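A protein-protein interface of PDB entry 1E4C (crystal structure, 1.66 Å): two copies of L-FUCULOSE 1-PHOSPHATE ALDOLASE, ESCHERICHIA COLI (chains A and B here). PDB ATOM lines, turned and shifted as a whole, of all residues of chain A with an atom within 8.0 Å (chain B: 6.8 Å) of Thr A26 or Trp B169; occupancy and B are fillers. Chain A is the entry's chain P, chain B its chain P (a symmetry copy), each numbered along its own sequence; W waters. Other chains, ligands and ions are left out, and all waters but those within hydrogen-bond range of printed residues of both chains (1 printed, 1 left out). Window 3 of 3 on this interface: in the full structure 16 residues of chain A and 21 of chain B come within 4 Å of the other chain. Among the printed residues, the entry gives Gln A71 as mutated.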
ATOM      1  N   ASN A  23      -1.415 -30.268 -26.744  1.00  0.00           N
ATOM      2  CA  ASN A  23      -0.933 -30.311 -25.373  1.00  0.00           C
ATOM      3  C   ASN A  23       0.541 -29.917 -25.369  1.00  0.00           C
ATOM      4  O   ASN A  23       1.354 -30.403 -26.146  1.00  0.00           O
ATOM      5  CB  ASN A  23      -1.118 -31.682 -24.714  1.00  0.00           C
ATOM      6  CG  ASN A  23      -0.644 -31.638 -23.267  1.00  0.00           C
ATOM      7  OD1 ASN A  23      -1.011 -30.722 -22.532  1.00  0.00           O
ATOM      8  ND2 ASN A  23       0.191 -32.577 -22.860  1.00  0.00           N
ATOM      9  N   GLN A  24       0.814 -28.988 -24.477  1.00  0.00           N
ATOM     10  CA  GLN A  24       2.163 -28.489 -24.263  1.00  0.00           C
ATOM     11  C   GLN A  24       2.423 -28.600 -22.758  1.00  0.00           C
ATOM     12  O   GLN A  24       1.528 -28.356 -21.938  1.00  0.00           O
ATOM     13  CB  GLN A  24       2.316 -27.058 -24.757  1.00  0.00           C
ATOM     14  CG  GLN A  24       1.085 -26.180 -24.646  1.00  0.00           C
ATOM     15  CD  GLN A  24       0.889 -25.565 -23.276  1.00  0.00           C
ATOM     16  OE1 GLN A  24      -0.225 -25.198 -22.887  1.00  0.00           O
ATOM     17  NE2 GLN A  24       1.973 -25.440 -22.511  1.00  0.00           N
ATOM     18  N   GLY A  25       3.628 -29.037 -22.426  1.00  0.00           N
ATOM     19  CA  GLY A  25       4.021 -29.164 -21.040  1.00  0.00           C
ATOM     20  C   GLY A  25       3.141 -30.072 -20.204  1.00  0.00           C
ATOM     21  O   GLY A  25       2.994 -31.268 -20.467  1.00  0.00           O
ATOM     22  N   THR A  26       2.608 -29.526 -19.106  1.00  0.00           N
ATOM     23  CA  THR A  26       1.844 -30.342 -18.165  1.00  0.00           C
ATOM     24  C   THR A  26       0.398 -29.884 -18.019  1.00  0.00           C
ATOM     25  O   THR A  26      -0.247 -30.242 -17.030  1.00  0.00           O
ATOM     26  CB  THR A  26       2.520 -30.279 -16.775  1.00  0.00           C
ATOM     27  OG1 THR A  26       2.607 -28.894 -16.398  1.00  0.00           O
ATOM     28  CG2 THR A  26       3.917 -30.890 -16.804  1.00  0.00           C
ATOM     29  N   ALA A  27      -0.102 -29.147 -19.003  1.00  0.00           N
ATOM     30  CA  ALA A  27      -1.451 -28.603 -18.922  1.00  0.00           C
ATOM     31  C   ALA A  27      -2.558 -29.630 -19.115  1.00  0.00           C
ATOM     32  O   ALA A  27      -3.641 -29.504 -18.532  1.00  0.00           O
ATOM     33  CB  ALA A  27      -1.596 -27.519 -19.999  1.00  0.00           C
ATOM     34  N   GLY A  28      -2.341 -30.614 -19.974  1.00  0.00           N
ATOM     35  CA  GLY A  28      -3.404 -31.572 -20.293  1.00  0.00           C
ATOM     36  C   GLY A  28      -3.496 -32.746 -19.342  1.00  0.00           C
ATOM     37  O   GLY A  28      -2.580 -33.081 -18.593  1.00  0.00           O
ATOM     38  N   ASN A  29      -4.669 -33.390 -19.332  1.00  0.00           N
ATOM     39  CA  ASN A  29      -4.885 -34.579 -18.511  1.00  0.00           C
ATOM     40  C   ASN A  29      -6.020 -35.355 -19.192  1.00  0.00           C
ATOM     41  O   ASN A  29      -6.840 -34.812 -19.940  1.00  0.00           O
ATOM     42  CB  ASN A  29      -5.209 -34.357 -17.046  1.00  0.00           C
ATOM     43  CG  ASN A  29      -6.026 -33.110 -16.755  1.00  0.00           C
ATOM     44  OD1 ASN A  29      -7.214 -33.069 -17.051  1.00  0.00           O
ATOM     45  ND2 ASN A  29      -5.355 -32.097 -16.203  1.00  0.00           N
ATOM     46  N   THR A  41      -4.460 -39.296 -15.405  1.00  0.00           N
ATOM     47  CA  THR A  41      -3.047 -38.937 -15.312  1.00  0.00           C
ATOM     48  C   THR A  41      -2.859 -37.941 -14.168  1.00  0.00           C
ATOM     49  O   THR A  41      -3.748 -37.146 -13.850  1.00  0.00           O
ATOM     50  CB  THR A  41      -2.591 -38.267 -16.626  1.00  0.00           C
ATOM     51  OG1 THR A  41      -3.470 -37.168 -16.914  1.00  0.00           O
ATOM     52  CG2 THR A  41      -2.670 -39.270 -17.771  1.00  0.00           C
ATOM     53  N   PRO A  42      -1.714 -37.972 -13.512  1.00  0.00           N
ATOM     54  CA  PRO A  42      -1.408 -37.086 -12.401  1.00  0.00           C
ATOM     55  C   PRO A  42      -0.921 -35.718 -12.860  1.00  0.00           C
ATOM     56  O   PRO A  42      -0.513 -35.541 -14.016  1.00  0.00           O
ATOM     57  CB  PRO A  42      -0.293 -37.826 -11.655  1.00  0.00           C
ATOM     58  CG  PRO A  42       0.418 -38.565 -12.735  1.00  0.00           C
ATOM     59  CD  PRO A  42      -0.593 -38.913 -13.793  1.00  0.00           C
ATOM     60  N   THR A  43      -0.981 -34.742 -11.968  1.00  0.00           N
ATOM     61  CA  THR A  43      -0.536 -33.387 -12.271  1.00  0.00           C
ATOM     62  C   THR A  43       0.990 -33.307 -12.264  1.00  0.00           C
ATOM     63  O   THR A  43       1.636 -33.937 -11.414  1.00  0.00           O
ATOM     64  CB  THR A  43      -1.061 -32.392 -11.215  1.00  0.00           C
ATOM     65  OG1 THR A  43      -2.493 -32.324 -11.297  1.00  0.00           O
ATOM     66  CG2 THR A  43      -0.512 -30.986 -11.430  1.00  0.00           C
ATOM     67  N   GLY A  44       1.543 -32.520 -13.181  1.00  0.00           N
ATOM     68  CA  GLY A  44       2.963 -32.254 -13.173  1.00  0.00           C
ATOM     69  C   GLY A  44       3.938 -33.238 -13.760  1.00  0.00           C
ATOM     70  O   GLY A  44       5.144 -32.936 -13.729  1.00  0.00           O
ATOM     71  N   ILE A  45       3.508 -34.383 -14.275  1.00  0.00           N
ATOM     72  CA  ILE A  45       4.462 -35.297 -14.911  1.00  0.00           C
ATOM     73  C   ILE A  45       4.339 -35.086 -16.417  1.00  0.00           C
ATOM     74  O   ILE A  45       3.268 -35.292 -16.981  1.00  0.00           O
ATOM     75  CB  ILE A  45       4.227 -36.769 -14.581  1.00  0.00           C
ATOM     76  CG1 ILE A  45       4.445 -36.997 -13.078  1.00  0.00           C
ATOM     77  CG2 ILE A  45       5.145 -37.682 -15.385  1.00  0.00           C
ATOM     78  CD1 ILE A  45       3.843 -38.318 -12.648  1.00  0.00           C
ATOM     79  N   PRO A  46       5.425 -34.647 -17.037  1.00  0.00           N
ATOM     80  CA  PRO A  46       5.442 -34.426 -18.473  1.00  0.00           C
ATOM     81  C   PRO A  46       5.098 -35.727 -19.182  1.00  0.00           C
ATOM     82  O   PRO A  46       5.458 -36.805 -18.696  1.00  0.00           O
ATOM     83  CB  PRO A  46       6.854 -33.964 -18.771  1.00  0.00           C
ATOM     84  CG  PRO A  46       7.678 -34.338 -17.592  1.00  0.00           C
ATOM     85  CD  PRO A  46       6.742 -34.391 -16.414  1.00  0.00           C
ATOM     86  N   TYR A  47       4.449 -35.632 -20.334  1.00  0.00           N
ATOM     87  CA  TYR A  47       4.030 -36.799 -21.092  1.00  0.00           C
ATOM     88  C   TYR A  47       5.133 -37.816 -21.331  1.00  0.00           C
ATOM     89  O   TYR A  47       4.916 -39.010 -21.114  1.00  0.00           O
ATOM     90  CB  TYR A  47       3.387 -36.380 -22.423  1.00  0.00           C
ATOM     91  CG  TYR A  47       4.368 -35.875 -23.458  1.00  0.00           C
ATOM     92  CD1 TYR A  47       4.889 -34.588 -23.375  1.00  0.00           C
ATOM     93  CD2 TYR A  47       4.791 -36.693 -24.500  1.00  0.00           C
ATOM     94  CE1 TYR A  47       5.795 -34.120 -24.310  1.00  0.00           C
ATOM     95  CE2 TYR A  47       5.696 -36.235 -25.442  1.00  0.00           C
ATOM     96  CZ  TYR A  47       6.192 -34.950 -25.340  1.00  0.00           C
ATOM     97  OH  TYR A  47       7.093 -34.488 -26.275  1.00  0.00           O
ATOM     98  N   GLU A  48       6.326 -37.396 -21.728  1.00  0.00           N
ATOM     99  CA  GLU A  48       7.436 -38.283 -22.025  1.00  0.00           C
ATOM    100  C   GLU A  48       7.972 -39.068 -20.839  1.00  0.00           C
ATOM    101  O   GLU A  48       8.621 -40.100 -21.074  1.00  0.00           O
ATOM    102  CB  GLU A  48       8.546 -37.500 -22.737  1.00  0.00           C
ATOM    103  CG  GLU A  48       9.515 -36.785 -21.816  1.00  0.00           C
ATOM    104  CD  GLU A  48       9.200 -35.317 -21.627  1.00  0.00           C
ATOM    105  OE1 GLU A  48       8.063 -34.880 -21.913  1.00  0.00           O
ATOM    106  OE2 GLU A  48      10.117 -34.586 -21.183  1.00  0.00           O
ATOM    107  N   GLN A  71      -3.972 -35.158  -8.695  1.00  0.00           N
ATOM    108  CA  GLN A  71      -4.457 -34.627  -9.973  1.00  0.00           C
ATOM    109  C   GLN A  71      -5.419 -33.505  -9.546  1.00  0.00           C
ATOM    110  O   GLN A  71      -6.579 -33.737  -9.227  1.00  0.00           O
ATOM    111  CB  GLN A  71      -5.110 -35.625 -10.902  1.00  0.00           C
ATOM    112  CG  GLN A  71      -5.865 -35.038 -12.093  1.00  0.00           C
ATOM    113  CD  GLN A  71      -5.080 -33.964 -12.809  1.00  0.00           C
ATOM    114  OE1 GLN A  71      -5.342 -32.771 -12.608  1.00  0.00           O
ATOM    115  NE2 GLN A  71      -4.105 -34.348 -13.619  1.00  0.00           N
ATOM    116  N   GLU A  73      -7.114 -31.283 -11.023  1.00  0.00           N
ATOM    117  CA  GLU A  73      -8.344 -31.034 -11.758  1.00  0.00           C
ATOM    118  C   GLU A  73      -9.250 -32.253 -11.847  1.00  0.00           C
ATOM    119  O   GLU A  73     -10.183 -32.290 -12.662  1.00  0.00           O
ATOM    120  CB  GLU A  73      -7.977 -30.570 -13.184  1.00  0.00           C
ATOM    121  CG  GLU A  73      -7.468 -29.125 -13.147  1.00  0.00           C
ATOM    122  CD  GLU A  73      -6.767 -28.750 -14.428  1.00  0.00           C
ATOM    123  OE1 GLU A  73      -5.850 -29.465 -14.860  1.00  0.00           O
ATOM    124  OE2 GLU A  73      -7.169 -27.721 -15.000  1.00  0.00           O
ATOM    125  N   HIS A  92      -8.812 -33.240 -21.398  1.00  0.00           N
ATOM    126  CA  HIS A  92      -8.732 -31.818 -21.039  1.00  0.00           C
ATOM    127  C   HIS A  92      -7.411 -31.247 -21.547  1.00  0.00           C
ATOM    128  O   HIS A  92      -6.378 -31.894 -21.396  1.00  0.00           O
ATOM    129  CB  HIS A  92      -8.772 -31.621 -19.522  1.00  0.00           C
ATOM    130  CG  HIS A  92      -8.475 -30.221 -19.071  1.00  0.00           C
ATOM    131  ND1 HIS A  92      -9.248 -29.138 -19.459  1.00  0.00           N
ATOM    132  CD2 HIS A  92      -7.478 -29.747 -18.287  1.00  0.00           C
ATOM    133  CE1 HIS A  92      -8.723 -28.046 -18.896  1.00  0.00           C
ATOM    134  NE2 HIS A  92      -7.662 -28.379 -18.189  1.00  0.00           N
ATOM    135  N   ASN A  93      -7.432 -30.054 -22.142  1.00  0.00           N
ATOM    136  CA  ASN A  93      -6.141 -29.456 -22.511  1.00  0.00           C
ATOM    137  C   ASN A  93      -6.337 -27.946 -22.549  1.00  0.00           C
ATOM    138  O   ASN A  93      -7.448 -27.467 -22.325  1.00  0.00           O
ATOM    139  CB  ASN A  93      -5.611 -29.989 -23.840  1.00  0.00           C
ATOM    140  CG  ASN A  93      -6.561 -29.744 -24.983  1.00  0.00           C
ATOM    141  OD1 ASN A  93      -7.082 -28.642 -25.166  1.00  0.00           O
ATOM    142  ND2 ASN A  93      -6.795 -30.781 -25.801  1.00  0.00           N
ATOM    143  N   HIS A  94      -5.243 -27.224 -22.771  1.00  0.00           N
ATOM    144  CA  HIS A  94      -5.273 -25.772 -22.865  1.00  0.00           C
ATOM    145  C   HIS A  94      -4.830 -25.428 -24.302  1.00  0.00           C
ATOM    146  O   HIS A  94      -3.992 -24.562 -24.501  1.00  0.00           O
ATOM    147  CB  HIS A  94      -4.384 -25.085 -21.839  1.00  0.00           C
ATOM    148  CG  HIS A  94      -4.689 -25.371 -20.399  1.00  0.00           C
ATOM    149  ND1 HIS A  94      -3.894 -24.835 -19.408  1.00  0.00           N
ATOM    150  CD2 HIS A  94      -5.661 -26.076 -19.765  1.00  0.00           C
ATOM    151  CE1 HIS A  94      -4.361 -25.224 -18.223  1.00  0.00           C
ATOM    152  NE2 HIS A  94      -5.436 -25.979 -18.416  1.00  0.00           N
ATOM    153  N   LEU B  20      10.559 -27.375 -29.502  1.00  0.00           N
ATOM    154  CA  LEU B  20       9.326 -26.720 -29.092  1.00  0.00           C
ATOM    155  C   LEU B  20       9.027 -25.492 -29.940  1.00  0.00           C
ATOM    156  O   LEU B  20       7.982 -24.874 -29.736  1.00  0.00           O
ATOM    157  CB  LEU B  20       9.370 -26.353 -27.602  1.00  0.00           C
ATOM    158  CG  LEU B  20       9.381 -27.546 -26.636  1.00  0.00           C
ATOM    159  CD1 LEU B  20       9.745 -27.107 -25.228  1.00  0.00           C
ATOM    160  CD2 LEU B  20       8.037 -28.273 -26.632  1.00  0.00           C
ATOM    161  N   VAL B  91      17.040 -19.145 -19.190  1.00  0.00           N
ATOM    162  CA  VAL B  91      16.798 -19.420 -20.606  1.00  0.00           C
ATOM    163  C   VAL B  91      16.512 -18.090 -21.302  1.00  0.00           C
ATOM    164  O   VAL B  91      15.661 -17.322 -20.827  1.00  0.00           O
ATOM    165  CB  VAL B  91      15.609 -20.391 -20.767  1.00  0.00           C
ATOM    166  CG1 VAL B  91      15.085 -20.431 -22.189  1.00  0.00           C
ATOM    167  CG2 VAL B  91      16.057 -21.784 -20.316  1.00  0.00           C
ATOM    168  N   MET B 114      -2.665 -19.305 -15.648  1.00  0.00           N
ATOM    169  CA  MET B 114      -1.291 -19.735 -15.670  1.00  0.00           C
ATOM    170  C   MET B 114      -0.290 -18.589 -15.655  1.00  0.00           C
ATOM    171  O   MET B 114       0.892 -18.859 -15.451  1.00  0.00           O
ATOM    172  CB  MET B 114      -1.003 -20.629 -16.881  1.00  0.00           C
ATOM    173  CG  MET B 114      -1.647 -22.009 -16.757  1.00  0.00           C
ATOM    174  SD  MET B 114      -0.868 -22.966 -15.435  1.00  0.00           S
ATOM    175  CE  MET B 114       0.825 -22.999 -16.017  1.00  0.00           C
ATOM    176  N   ALA B 117       2.325 -18.584 -12.779  1.00  0.00           N
ATOM    177  CA  ALA B 117       3.541 -19.367 -12.810  1.00  0.00           C
ATOM    178  C   ALA B 117       4.792 -18.500 -12.773  1.00  0.00           C
ATOM    179  O   ALA B 117       5.824 -18.974 -12.284  1.00  0.00           O
ATOM    180  CB  ALA B 117       3.612 -20.270 -14.042  1.00  0.00           C
ATOM    181  N   ALA B 118       4.736 -17.251 -13.225  1.00  0.00           N
ATOM    182  CA  ALA B 118       5.888 -16.357 -13.220  1.00  0.00           C
ATOM    183  C   ALA B 118       5.970 -15.513 -11.957  1.00  0.00           C
ATOM    184  O   ALA B 118       6.833 -14.642 -11.800  1.00  0.00           O
ATOM    185  CB  ALA B 118       5.890 -15.504 -14.479  1.00  0.00           C
ATOM    186  N   GLU B 161      14.545 -20.146 -13.339  1.00  0.00           N
ATOM    187  CA  GLU B 161      13.867 -21.027 -12.399  1.00  0.00           C
ATOM    188  C   GLU B 161      14.916 -21.863 -11.660  1.00  0.00           C
ATOM    189  O   GLU B 161      16.116 -21.668 -11.867  1.00  0.00           O
ATOM    190  CB  GLU B 161      12.872 -21.957 -13.092  1.00  0.00           C
ATOM    191  CG  GLU B 161      11.406 -21.663 -12.848  1.00  0.00           C
ATOM    192  CD  GLU B 161      10.952 -21.927 -11.429  1.00  0.00           C
ATOM    193  OE1 GLU B 161      11.760 -22.357 -10.571  1.00  0.00           O
ATOM    194  OE2 GLU B 161       9.762 -21.680 -11.127  1.00  0.00           O
ATOM    195  N   LEU B 164      16.999 -26.375 -15.040  1.00  0.00           N
ATOM    196  CA  LEU B 164      16.859 -26.205 -16.473  1.00  0.00           C
ATOM    197  C   LEU B 164      15.501 -26.638 -17.007  1.00  0.00           C
ATOM    198  O   LEU B 164      14.912 -25.965 -17.855  1.00  0.00           O
ATOM    199  CB  LEU B 164      17.940 -27.017 -17.204  1.00  0.00           C
ATOM    200  CG  LEU B 164      19.294 -26.325 -17.316  1.00  0.00           C
ATOM    201  CD1 LEU B 164      20.370 -27.328 -17.715  1.00  0.00           C
ATOM    202  CD2 LEU B 164      19.235 -25.170 -18.302  1.00  0.00           C
ATOM    203  N   GLU B 165      14.986 -27.752 -16.491  1.00  0.00           N
ATOM    204  CA  GLU B 165      13.687 -28.243 -16.934  1.00  0.00           C
ATOM    205  C   GLU B 165      12.571 -27.266 -16.606  1.00  0.00           C
ATOM    206  O   GLU B 165      11.712 -27.017 -17.467  1.00  0.00           O
ATOM    207  CB  GLU B 165      13.380 -29.614 -16.330  1.00  0.00           C
ATOM    208  CG  GLU B 165      14.200 -30.720 -16.987  1.00  0.00           C
ATOM    209  CD  GLU B 165      13.911 -32.030 -16.254  1.00  0.00           C
ATOM    210  OE1 GLU B 165      12.741 -32.470 -16.317  1.00  0.00           O
ATOM    211  OE2 GLU B 165      14.861 -32.542 -15.616  1.00  0.00           O
ATOM    212  N   LYS B 166      12.576 -26.733 -15.387  1.00  0.00           N
ATOM    213  CA  LYS B 166      11.528 -25.790 -15.001  1.00  0.00           C
ATOM    214  C   LYS B 166      11.716 -24.456 -15.726  1.00  0.00           C
ATOM    215  O   LYS B 166      10.712 -23.816 -16.041  1.00  0.00           O
ATOM    216  CB  LYS B 166      11.479 -25.546 -13.496  1.00  0.00           C
ATOM    217  CG  LYS B 166      10.323 -26.251 -12.812  1.00  0.00           C
ATOM    218  CD  LYS B 166       9.787 -25.478 -11.617  1.00  0.00           C
ATOM    219  CE  LYS B 166      10.023 -26.221 -10.308  1.00  0.00           C
ATOM    220  NZ  LYS B 166      10.295 -27.678 -10.484  1.00  0.00           N
ATOM    221  N   ALA B 167      12.968 -24.067 -15.977  1.00  0.00           N
ATOM    222  CA  ALA B 167      13.174 -22.804 -16.703  1.00  0.00           C
ATOM    223  C   ALA B 167      12.642 -22.924 -18.131  1.00  0.00           C
ATOM    224  O   ALA B 167      12.034 -21.990 -18.659  1.00  0.00           O
ATOM    225  CB  ALA B 167      14.636 -22.388 -16.716  1.00  0.00           C
ATOM    226  N   LEU B 168      12.897 -24.053 -18.804  1.00  0.00           N
ATOM    227  CA  LEU B 168      12.388 -24.210 -20.174  1.00  0.00           C
ATOM    228  C   LEU B 168      10.869 -24.278 -20.187  1.00  0.00           C
ATOM    229  O   LEU B 168      10.173 -23.690 -21.018  1.00  0.00           O
ATOM    230  CB  LEU B 168      13.001 -25.471 -20.813  1.00  0.00           C
ATOM    231  CG  LEU B 168      12.522 -25.736 -22.249  1.00  0.00           C
ATOM    232  CD1 LEU B 168      12.833 -24.555 -23.162  1.00  0.00           C
ATOM    233  CD2 LEU B 168      13.159 -27.006 -22.790  1.00  0.00           C
ATOM    234  N   TRP B 169      10.305 -25.008 -19.221  1.00  0.00           N
ATOM    235  CA  TRP B 169       8.864 -25.176 -19.061  1.00  0.00           C
ATOM    236  C   TRP B 169       8.207 -23.804 -18.903  1.00  0.00           C
ATOM    237  O   TRP B 169       7.217 -23.482 -19.560  1.00  0.00           O
ATOM    238  CB  TRP B 169       8.576 -26.072 -17.839  1.00  0.00           C
ATOM    239  CG  TRP B 169       7.118 -26.096 -17.471  1.00  0.00           C
ATOM    240  CD1 TRP B 169       6.157 -26.928 -17.988  1.00  0.00           C
ATOM    241  CD2 TRP B 169       6.453 -25.233 -16.540  1.00  0.00           C
ATOM    242  NE1 TRP B 169       4.936 -26.630 -17.420  1.00  0.00           N
ATOM    243  CE2 TRP B 169       5.097 -25.595 -16.529  1.00  0.00           C
ATOM    244  CE3 TRP B 169       6.886 -24.199 -15.702  1.00  0.00           C
ATOM    245  CZ2 TRP B 169       4.160 -24.956 -15.713  1.00  0.00           C
ATOM    246  CZ3 TRP B 169       5.959 -23.552 -14.905  1.00  0.00           C
ATOM    247  CH2 TRP B 169       4.611 -23.940 -14.921  1.00  0.00           C
ATOM    248  N   LEU B 170       8.802 -22.947 -18.069  1.00  0.00           N
ATOM    249  CA  LEU B 170       8.286 -21.597 -17.867  1.00  0.00           C
ATOM    250  C   LEU B 170       8.381 -20.762 -19.140  1.00  0.00           C
ATOM    251  O   LEU B 170       7.422 -20.067 -19.513  1.00  0.00           O
ATOM    252  CB  LEU B 170       9.022 -20.904 -16.709  1.00  0.00           C
ATOM    253  CG  LEU B 170       8.593 -19.465 -16.395  1.00  0.00           C
ATOM    254  CD1 LEU B 170       7.127 -19.378 -16.023  1.00  0.00           C
ATOM    255  CD2 LEU B 170       9.453 -18.873 -15.286  1.00  0.00           C
ATOM    256  N   ALA B 171       9.501 -20.836 -19.842  1.00  0.00           N
ATOM    257  CA  ALA B 171       9.691 -20.095 -21.093  1.00  0.00           C
ATOM    258  C   ALA B 171       8.605 -20.470 -22.101  1.00  0.00           C
ATOM    259  O   ALA B 171       8.030 -19.614 -22.773  1.00  0.00           O
ATOM    260  CB  ALA B 171      11.060 -20.391 -21.680  1.00  0.00           C
ATOM    261  N   HIS B 172       8.297 -21.766 -22.170  1.00  0.00           N
ATOM    262  CA  HIS B 172       7.241 -22.218 -23.070  1.00  0.00           C
ATOM    263  C   HIS B 172       5.877 -21.712 -22.627  1.00  0.00           C
ATOM    264  O   HIS B 172       5.106 -21.262 -23.477  1.00  0.00           O
ATOM    265  CB  HIS B 172       7.219 -23.754 -23.128  1.00  0.00           C
ATOM    266  CG  HIS B 172       6.180 -24.224 -24.107  1.00  0.00           C
ATOM    267  ND1 HIS B 172       6.412 -24.239 -25.464  1.00  0.00           N
ATOM    268  CD2 HIS B 172       4.909 -24.660 -23.927  1.00  0.00           C
ATOM    269  CE1 HIS B 172       5.334 -24.687 -26.086  1.00  0.00           C
ATOM    270  NE2 HIS B 172       4.413 -24.946 -25.176  1.00  0.00           N
ATOM    271  N   GLU B 173       5.569 -21.738 -21.327  1.00  0.00           N
ATOM    272  CA  GLU B 173       4.283 -21.230 -20.862  1.00  0.00           C
ATOM    273  C   GLU B 173       4.155 -19.735 -21.183  1.00  0.00           C
ATOM    274  O   GLU B 173       3.054 -19.278 -21.511  1.00  0.00           O
ATOM    275  CB  GLU B 173       4.063 -21.437 -19.363  1.00  0.00           C
ATOM    276  CG  GLU B 173       3.850 -22.871 -18.906  1.00  0.00           C
ATOM    277  CD  GLU B 173       2.653 -23.530 -19.576  1.00  0.00           C
ATOM    278  OE1 GLU B 173       1.556 -22.930 -19.592  1.00  0.00           O
ATOM    279  OE2 GLU B 173       2.827 -24.646 -20.120  1.00  0.00           O
ATOM    280  N   VAL B 174       5.244 -18.978 -21.091  1.00  0.00           N
ATOM    281  CA  VAL B 174       5.164 -17.540 -21.395  1.00  0.00           C
ATOM    282  C   VAL B 174       4.928 -17.356 -22.881  1.00  0.00           C
ATOM    283  O   VAL B 174       4.150 -16.481 -23.291  1.00  0.00           O
ATOM    284  CB  VAL B 174       6.392 -16.768 -20.905  1.00  0.00           C
ATOM    285  CG1 VAL B 174       6.292 -15.291 -21.283  1.00  0.00           C
ATOM    286  CG2 VAL B 174       6.547 -16.880 -19.388  1.00  0.00           C
ATOM    287  N   PHE B 206      -0.814 -22.720  -6.194  1.00  0.00           N
ATOM    288  CA  PHE B 206       0.399 -23.158  -6.868  1.00  0.00           C
ATOM    289  C   PHE B 206       1.554 -23.503  -5.939  1.00  0.00           C
ATOM    290  O   PHE B 206       1.608 -22.980  -4.801  1.00  0.00           O
ATOM    291  CB  PHE B 206       0.857 -22.081  -7.864  1.00  0.00           C
ATOM    292  CG  PHE B 206       0.162 -22.083  -9.197  1.00  0.00           C
ATOM    293  CD1 PHE B 206      -0.842 -22.977  -9.517  1.00  0.00           C
ATOM    294  CD2 PHE B 206       0.544 -21.162 -10.159  1.00  0.00           C
ATOM    295  CE1 PHE B 206      -1.463 -22.963 -10.750  1.00  0.00           C
ATOM    296  CE2 PHE B 206      -0.062 -21.132 -11.397  1.00  0.00           C
ATOM    297  CZ  PHE B 206      -1.070 -22.030 -11.689  1.00  0.00           C
HETATM  298  O   HOH W   1      -1.504 -23.486 -19.971  1.00  0.00           O
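The side-chain carboxylate (OE2) of Glu B173 sits at hydrogen-bond distance from the side-chain amide nitrogen (NE2) of Gln A24. OG1 of Thr A26 sits at hydrogen-bond distance from NE1 of Trp B169 (3.4 Å).
Water W1 lies within hydrogen-bond range of a ring nitrogen (ND1) of His A94 (2.8 Å) and the side-chain carboxylate of Glu B173 (3.1 Å).
Gln A24 touches His B172.
No position is printed for both chains. Of the 3 pairs that touch across the chains among the printed residues, none has its exchanged pair printed and touching as well.
Of chain B, only Trp B169 comes within 4 Å of Thr A26. Trp B169 touches just one residue of chain A: Thr A26 (3.4 Å). Of the printed residues of chain B, Gln A24 touches His B172 and Glu B173. Printed residues of chain A within 4 Å of His B172: Gln A24. Of the printed residues of chain A, Glu B173 touches Gln A24. The nearest residue of chain B that does not touch Thr A26 is Glu B173 (5.0 Å). The nearest residue of chain A that does not touch Trp B169 is Gly A25 (4.3 Å).
Hydrophobic or aromatic side chains of chain B that line the printed part of chain A: Trp B169 and His B172. Of the 20 printed residues of chain A, 2 touch a printed residue of chain B.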
